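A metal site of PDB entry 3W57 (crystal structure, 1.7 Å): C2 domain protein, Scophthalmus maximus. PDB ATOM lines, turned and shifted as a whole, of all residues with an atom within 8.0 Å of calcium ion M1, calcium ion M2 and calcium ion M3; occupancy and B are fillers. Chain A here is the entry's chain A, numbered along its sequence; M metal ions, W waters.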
ATOM      1  N   SER A  36      -8.436  22.013   4.420  1.00  0.00           N
ATOM      2  CA  SER A  36      -8.856  21.402   3.169  1.00  0.00           C
ATOM      3  C   SER A  36      -7.642  21.035   2.310  1.00  0.00           C
ATOM      4  O   SER A  36      -6.609  21.694   2.353  1.00  0.00           O
ATOM      5  CB  SER A  36      -9.735  22.396   2.388  1.00  0.00           C
ATOM      6  OG  SER A  36     -10.251  21.844   1.179  1.00  0.00           O
ATOM      7  N   ASP A  37      -7.781  19.966   1.539  1.00  0.00           N
ATOM      8  CA  ASP A  37      -6.858  19.617   0.468  1.00  0.00           C
ATOM      9  C   ASP A  37      -7.224  20.504  -0.740  1.00  0.00           C
ATOM     10  O   ASP A  37      -8.201  21.252  -0.711  1.00  0.00           O
ATOM     11  CB  ASP A  37      -7.064  18.128   0.121  1.00  0.00           C
ATOM     12  CG  ASP A  37      -5.861  17.494  -0.538  1.00  0.00           C
ATOM     13  OD1 ASP A  37      -4.915  18.216  -0.880  1.00  0.00           O
ATOM     14  OD2 ASP A  37      -5.894  16.261  -0.723  1.00  0.00           O
ATOM     15  N   LEU A  38      -6.423  20.424  -1.792  1.00  0.00           N
ATOM     16  CA  LEU A  38      -6.756  21.097  -3.047  1.00  0.00           C
ATOM     17  C   LEU A  38      -8.119  20.610  -3.544  1.00  0.00           C
ATOM     18  O   LEU A  38      -8.931  21.377  -4.054  1.00  0.00           O
ATOM     19  CB  LEU A  38      -5.671  20.790  -4.074  1.00  0.00           C
ATOM     20  CG  LEU A  38      -5.897  21.202  -5.536  1.00  0.00           C
ATOM     21  CD1 LEU A  38      -6.340  22.651  -5.653  1.00  0.00           C
ATOM     22  CD2 LEU A  38      -4.609  20.958  -6.322  1.00  0.00           C
ATOM     23  N   MET A  39      -8.365  19.314  -3.386  1.00  0.00           N
ATOM     24  CA  MET A  39      -9.659  18.747  -3.728  1.00  0.00           C
ATOM     25  C   MET A  39     -10.175  17.881  -2.601  1.00  0.00           C
ATOM     26  O   MET A  39      -9.859  16.693  -2.536  1.00  0.00           O
ATOM     27  CB  MET A  39      -9.539  17.908  -4.997  1.00  0.00           C
ATOM     28  CG  MET A  39      -9.150  18.729  -6.193  1.00  0.00           C
ATOM     29  SD  MET A  39      -9.051  17.708  -7.660  1.00  0.00           S
ATOM     30  CE  MET A  39      -7.596  16.732  -7.292  1.00  0.00           C
ATOM     31  N   GLY A  40     -10.958  18.485  -1.722  1.00  0.00           N
ATOM     32  CA  GLY A  40     -11.674  17.726  -0.724  1.00  0.00           C
ATOM     33  C   GLY A  40     -10.902  17.545   0.566  1.00  0.00           C
ATOM     34  O   GLY A  40     -10.045  18.347   0.908  1.00  0.00           O
ATOM     35  N   ILE A  41     -11.197  16.454   1.269  1.00  0.00           N
ATOM     36  CA  ILE A  41     -10.690  16.272   2.621  1.00  0.00           C
ATOM     37  C   ILE A  41      -9.293  15.673   2.610  1.00  0.00           C
ATOM     38  O   ILE A  41      -9.008  14.773   1.834  1.00  0.00           O
ATOM     39  CB  ILE A  41     -11.662  15.409   3.446  1.00  0.00           C
ATOM     40  CG1 ILE A  41     -13.057  16.045   3.391  1.00  0.00           C
ATOM     41  CG2 ILE A  41     -11.182  15.238   4.880  1.00  0.00           C
ATOM     42  CD1 ILE A  41     -14.146  15.226   4.058  1.00  0.00           C
ATOM     43  N   THR A  42      -8.429  16.201   3.454  1.00  0.00           N
ATOM     44  CA  THR A  42      -7.027  15.800   3.531  1.00  0.00           C
ATOM     45  C   THR A  42      -6.811  14.316   3.888  1.00  0.00           C
ATOM     46  O   THR A  42      -7.639  13.681   4.567  1.00  0.00           O
ATOM     47  CB  THR A  42      -6.291  16.722   4.515  1.00  0.00           C
ATOM     48  OG1 THR A  42      -6.250  18.034   3.963  1.00  0.00           O
ATOM     49  CG2 THR A  42      -4.878  16.270   4.797  1.00  0.00           C
ATOM     50  N   ASP A  43      -5.687  13.780   3.415  1.00  0.00           N
ATOM     51  CA  ASP A  43      -5.348  12.361   3.525  1.00  0.00           C
ATOM     52  C   ASP A  43      -4.038  12.239   4.288  1.00  0.00           C
ATOM     53  O   ASP A  43      -2.963  12.014   3.711  1.00  0.00           O
ATOM     54  CB  ASP A  43      -5.229  11.812   2.110  1.00  0.00           C
ATOM     55  CG  ASP A  43      -6.387  12.264   1.252  1.00  0.00           C
ATOM     56  OD1 ASP A  43      -7.503  11.777   1.517  1.00  0.00           O
ATOM     57  OD2 ASP A  43      -6.208  13.136   0.371  1.00  0.00           O
ATOM     58  N   GLY A  44      -4.121  12.412   5.601  1.00  0.00           N
ATOM     59  CA  GLY A  44      -2.933  12.573   6.419  1.00  0.00           C
ATOM     60  C   GLY A  44      -2.169  11.315   6.761  1.00  0.00           C
ATOM     61  O   GLY A  44      -2.748  10.233   6.910  1.00  0.00           O
ATOM     62  N   VAL A  60      -1.934   5.973   5.621  1.00  0.00           N
ATOM     63  CA  VAL A  60      -2.680   7.173   5.270  1.00  0.00           C
ATOM     64  C   VAL A  60      -4.101   7.017   5.795  1.00  0.00           C
ATOM     65  O   VAL A  60      -4.737   5.951   5.630  1.00  0.00           O
ATOM     66  CB  VAL A  60      -2.697   7.368   3.731  1.00  0.00           C
ATOM     67  CG1 VAL A  60      -3.560   8.551   3.347  1.00  0.00           C
ATOM     68  CG2 VAL A  60      -1.283   7.552   3.189  1.00  0.00           C
ATOM     69  N   ASN A  61      -4.583   8.058   6.468  1.00  0.00           N
ATOM     70  CA  ASN A  61      -5.943   8.066   6.982  1.00  0.00           C
ATOM     71  C   ASN A  61      -6.765   8.891   6.004  1.00  0.00           C
ATOM     72  O   ASN A  61      -6.847  10.112   6.099  1.00  0.00           O
ATOM     73  CB  ASN A  61      -5.957   8.658   8.407  1.00  0.00           C
ATOM     74  CG  ASN A  61      -7.207   8.282   9.171  1.00  0.00           C
ATOM     75  OD1 ASN A  61      -8.285   8.285   8.620  1.00  0.00           O
ATOM     76  ND2 ASN A  61      -7.045   7.960  10.456  1.00  0.00           N
ATOM     77  N   HIS A  62      -7.331   8.217   5.004  1.00  0.00           N
ATOM     78  CA  HIS A  62      -7.929   8.894   3.861  1.00  0.00           C
ATOM     79  C   HIS A  62      -9.164   9.709   4.198  1.00  0.00           C
ATOM     80  O   HIS A  62      -9.992   9.276   5.006  1.00  0.00           O
ATOM     81  CB  HIS A  62      -8.294   7.885   2.775  1.00  0.00           C
ATOM     82  CG  HIS A  62      -7.101   7.220   2.160  1.00  0.00           C
ATOM     83  ND1 HIS A  62      -6.377   7.813   1.144  1.00  0.00           N
ATOM     84  CD2 HIS A  62      -6.471   6.052   2.445  1.00  0.00           C
ATOM     85  CE1 HIS A  62      -5.370   7.013   0.809  1.00  0.00           C
ATOM     86  NE2 HIS A  62      -5.413   5.952   1.581  1.00  0.00           N
ATOM     87  N   ASN A  63      -9.227  10.891   3.599  1.00  0.00           N
ATOM     88  CA  ASN A  63     -10.423  11.735   3.675  1.00  0.00           C
ATOM     89  C   ASN A  63     -10.901  11.927   5.106  1.00  0.00           C
ATOM     90  O   ASN A  63     -12.076  11.688   5.414  1.00  0.00           O
ATOM     91  CB  ASN A  63     -11.514  11.128   2.824  1.00  0.00           C
ATOM     92  CG  ASN A  63     -11.113  11.040   1.392  1.00  0.00           C
ATOM     93  OD1 ASN A  63     -10.609  12.009   0.842  1.00  0.00           O
ATOM     94  ND2 ASN A  63     -11.284   9.861   0.774  1.00  0.00           N
ATOM     95  N   ASN A  64      -9.981  12.366   5.947  1.00  0.00           N
ATOM     96  CA  ASN A  64     -10.256  12.533   7.360  1.00  0.00           C
ATOM     97  C   ASN A  64      -9.611  13.823   7.876  1.00  0.00           C
ATOM     98  O   ASN A  64      -8.394  13.939   7.901  1.00  0.00           O
ATOM     99  CB  ASN A  64      -9.727  11.306   8.122  1.00  0.00           C
ATOM    100  CG  ASN A  64     -10.275  11.194   9.550  1.00  0.00           C
ATOM    101  OD1 ASN A  64     -10.751  12.174  10.120  1.00  0.00           O
ATOM    102  ND2 ASN A  64     -10.168   9.992  10.134  1.00  0.00           N
ATOM    103  N   HIS A  89       2.033  14.874   6.811  1.00  0.00           N
ATOM    104  CA  HIS A  89       1.938  15.076   5.369  1.00  0.00           C
ATOM    105  C   HIS A  89       0.543  14.738   4.888  1.00  0.00           C
ATOM    106  O   HIS A  89      -0.149  13.927   5.493  1.00  0.00           O
ATOM    107  CB  HIS A  89       2.892  14.147   4.608  1.00  0.00           C
ATOM    108  CG  HIS A  89       4.349  14.370   4.896  1.00  0.00           C
ATOM    109  ND1 HIS A  89       5.209  14.928   3.970  1.00  0.00           N
ATOM    110  CD2 HIS A  89       5.104  14.070   5.977  1.00  0.00           C
ATOM    111  CE1 HIS A  89       6.425  14.973   4.476  1.00  0.00           C
ATOM    112  NE2 HIS A  89       6.399  14.462   5.695  1.00  0.00           N
ATOM    113  N   ASP A  90       0.162  15.356   3.766  1.00  0.00           N
ATOM    114  CA  ASP A  90      -1.016  14.931   3.002  1.00  0.00           C
ATOM    115  C   ASP A  90      -0.551  14.078   1.823  1.00  0.00           C
ATOM    116  O   ASP A  90       0.267  14.541   1.026  1.00  0.00           O
ATOM    117  CB  ASP A  90      -1.760  16.135   2.466  1.00  0.00           C
ATOM    118  CG  ASP A  90      -2.811  15.765   1.441  1.00  0.00           C
ATOM    119  OD1 ASP A  90      -3.681  14.925   1.749  1.00  0.00           O
ATOM    120  OD2 ASP A  90      -2.748  16.251   0.293  1.00  0.00           O
ATOM    121  N   GLU A  91      -1.083  12.858   1.693  1.00  0.00           N
ATOM    122  CA  GLU A  91      -0.791  12.058   0.513  1.00  0.00           C
ATOM    123  C   GLU A  91      -1.537  12.589  -0.702  1.00  0.00           C
ATOM    124  O   GLU A  91      -2.741  12.832  -0.633  1.00  0.00           O
ATOM    125  CB  GLU A  91      -1.167  10.583   0.738  1.00  0.00           C
ATOM    126  CG  GLU A  91      -0.714   9.688  -0.404  1.00  0.00           C
ATOM    127  CD  GLU A  91      -1.322   8.295  -0.354  1.00  0.00           C
ATOM    128  OE1 GLU A  91      -0.549   7.321  -0.242  1.00  0.00           O
ATOM    129  OE2 GLU A  91      -2.563   8.177  -0.438  1.00  0.00           O
ATOM    130  N   ASP A  92      -0.807  12.777  -1.799  1.00  0.00           N
ATOM    131  CA  ASP A  92      -1.401  13.149  -3.081  1.00  0.00           C
ATOM    132  C   ASP A  92      -0.816  12.296  -4.196  1.00  0.00           C
ATOM    133  O   ASP A  92       0.185  11.597  -4.010  1.00  0.00           O
ATOM    134  CB  ASP A  92      -1.106  14.602  -3.392  1.00  0.00           C
ATOM    135  CG  ASP A  92      -2.115  15.563  -2.781  1.00  0.00           C
ATOM    136  OD1 ASP A  92      -3.316  15.233  -2.684  1.00  0.00           O
ATOM    137  OD2 ASP A  92      -1.668  16.661  -2.454  1.00  0.00           O
ATOM    138  N   THR A  93      -1.461  12.339  -5.356  1.00  0.00           N
ATOM    139  CA  THR A  93      -1.041  11.498  -6.490  1.00  0.00           C
ATOM    140  C   THR A  93       0.372  11.799  -7.003  1.00  0.00           C
ATOM    141  O   THR A  93       1.147  10.863  -7.271  1.00  0.00           O
ATOM    142  CB  THR A  93      -2.057  11.578  -7.624  1.00  0.00           C
ATOM    143  OG1 THR A  93      -3.313  11.047  -7.157  1.00  0.00           O
ATOM    144  CG2 THR A  93      -1.590  10.746  -8.810  1.00  0.00           C
ATOM    145  N   PHE A  95       2.675  14.759  -5.835  1.00  0.00           N
ATOM    146  CA  PHE A  95       3.607  15.251  -4.810  1.00  0.00           C
ATOM    147  C   PHE A  95       2.872  15.345  -3.488  1.00  0.00           C
ATOM    148  O   PHE A  95       1.866  16.026  -3.402  1.00  0.00           O
ATOM    149  CB  PHE A  95       4.143  16.649  -5.133  1.00  0.00           C
ATOM    150  CG  PHE A  95       4.828  16.748  -6.480  1.00  0.00           C
ATOM    151  CD1 PHE A  95       6.183  16.513  -6.603  1.00  0.00           C
ATOM    152  CD2 PHE A  95       4.096  17.083  -7.603  1.00  0.00           C
ATOM    153  CE1 PHE A  95       6.806  16.613  -7.850  1.00  0.00           C
ATOM    154  CE2 PHE A  95       4.703  17.188  -8.852  1.00  0.00           C
ATOM    155  CZ  PHE A  95       6.048  16.961  -8.970  1.00  0.00           C
ATOM    156  N   ASP A  96       3.384  14.685  -2.442  1.00  0.00           N
ATOM    157  CA  ASP A  96       2.772  14.837  -1.116  1.00  0.00           C
ATOM    158  C   ASP A  96       3.103  16.216  -0.556  1.00  0.00           C
ATOM    159  O   ASP A  96       4.189  16.756  -0.828  1.00  0.00           O
ATOM    160  CB  ASP A  96       3.280  13.760  -0.151  1.00  0.00           C
ATOM    161  CG  ASP A  96       2.813  12.371  -0.499  1.00  0.00           C
ATOM    162  OD1 ASP A  96       2.010  12.209  -1.443  1.00  0.00           O
ATOM    163  OD2 ASP A  96       3.239  11.410   0.178  1.00  0.00           O
ATOM    164  N   ASP A  97       2.190  16.792   0.225  1.00  0.00           N
ATOM    165  CA  ASP A  97       2.385  18.121   0.801  1.00  0.00           C
ATOM    166  C   ASP A  97       2.701  18.011   2.291  1.00  0.00           C
ATOM    167  O   ASP A  97       1.956  17.376   3.036  1.00  0.00           O
ATOM    168  CB  ASP A  97       1.128  18.967   0.649  1.00  0.00           C
ATOM    169  CG  ASP A  97       0.860  19.338  -0.780  1.00  0.00           C
ATOM    170  OD1 ASP A  97       1.775  19.897  -1.422  1.00  0.00           O
ATOM    171  OD2 ASP A  97      -0.247  19.033  -1.273  1.00  0.00           O
ATOM    172  N   LEU A  98       3.774  18.665   2.710  1.00  0.00           N
ATOM    173  CA  LEU A  98       4.120  18.673   4.125  1.00  0.00           C
ATOM    174  C   LEU A  98       3.340  19.783   4.810  1.00  0.00           C
ATOM    175  O   LEU A  98       3.470  20.962   4.454  1.00  0.00           O
ATOM    176  CB  LEU A  98       5.645  18.831   4.289  1.00  0.00           C
ATOM    177  CG  LEU A  98       6.226  18.919   5.705  1.00  0.00           C
ATOM    178  CD1 LEU A  98       5.652  17.862   6.652  1.00  0.00           C
ATOM    179  CD2 LEU A  98       7.720  18.794   5.634  1.00  0.00           C
ATOM    180  N   LEU A  99       2.489  19.399   5.777  1.00  0.00           N
ATOM    181  CA  LEU A  99       1.593  20.345   6.423  1.00  0.00           C
ATOM    182  C   LEU A  99       2.166  20.961   7.684  1.00  0.00           C
ATOM    183  O   LEU A  99       1.808  22.083   8.039  1.00  0.00           O
ATOM    184  CB  LEU A  99       0.258  19.682   6.745  1.00  0.00           C
ATOM    185  CG  LEU A  99      -0.436  18.936   5.606  1.00  0.00           C
ATOM    186  CD1 LEU A  99      -1.759  18.376   6.095  1.00  0.00           C
ATOM    187  CD2 LEU A  99      -0.665  19.834   4.406  1.00  0.00           C
HETATM  188 CA    CA M   1      -4.416  14.479  -0.632  1.00  0.00          CA
HETATM  189 CA    CA M   2      -2.502  18.377  -1.063  1.00  0.00          CA
HETATM  190 CA    CA M   3      -8.772  13.246   0.021  1.00  0.00          CA
HETATM  191  O   HOH W   1      -8.072  11.666  -1.728  1.00  0.00           O
HETATM  192  O   HOH W   2      -5.602  13.201  -2.523  1.00  0.00           O
HETATM  193  O   HOH W   3     -10.697  13.596  -1.489  1.00  0.00           O
HETATM  194  O   HOH W   4      -2.200  19.314   1.232  1.00  0.00           O
HETATM  195  O   HOH W   5      -3.197  20.793  -1.132  1.00  0.00           O
HETATM  196  O   HOH W   6      -8.211  15.158  -1.378  1.00  0.00           O
HETATM  197  O   HOH W   7      -2.691  19.220  -3.517  1.00  0.00           O
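Of the 24 residues printed, 3 come within 4 Å of calcium ion M3.
The side-chain hydroxyl (OG1) of Thr 42 lies within hydrogen-bond range of the backbone NH (N) of Asp 37, at 3.5 Å.
The side-chain carboxylate of Asp 96 lies within hydrogen-bond range of the backbone NH of Asp 92 (2.9 Å).
The backbone carbonyl oxygen (O) of Thr 42 lies within hydrogen-bond range of the backbone NH (N) of Asn 63 (3.4 Å).
Along chain A the residues within 4 Å of calcium ion M2 span positions 37 to 97.
Calcium ion M3 is bound by OD1 of Asn 63 (2.4 Å), O of Ile 41 (2.4 Å), water W6 (2.4 Å), OD1 of Asp 43 (2.5 Å), water W1 (2.5 Å), water W3 (2.5 Å) and OD2 of Asp 43 (2.6 Å).
Within 4 Å of calcium ion M1: Asp 37, Asp 43, Asp 90, Glu 91 and Asp 92.
OD2 of Asp 97 binds calcium ion M2 (2.4 Å).
OD2 of Asp 92 is bound to calcium ion M2 (2.4 Å).
Calcium ion M2 is bound by OD1 of Asp 37 (2.4 Å).
Water W4 is bound to calcium ion M2 (2.5 Å).
Water W5 binds calcium ion M2.
Calcium ion M2 is bound by the side-chain carboxylate (OD2) of Asp 90, 2.5 Å away.
Calcium ion M2 is bound by water W7, 2.6 Å away.
Calcium ion M1 is bound by the side-chain carboxylate (OD2) of Asp 37 (2.3 Å), the backbone carbonyl oxygen (O) of Glu 91 (2.3 Å), the side-chain carboxylate (OD1) of Asp 92 (2.4 Å), the side-chain carboxylate (OD2) of Asp 43 (2.5 Å), the side-chain carboxylate (OD1) of Asp 90 (2.5 Å), water W2 (2.6 Å) and the side-chain carboxylate (OD2) of Asp 90 (2.6 Å).
Calcium ion M1 has seven donor atoms within binding distance.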
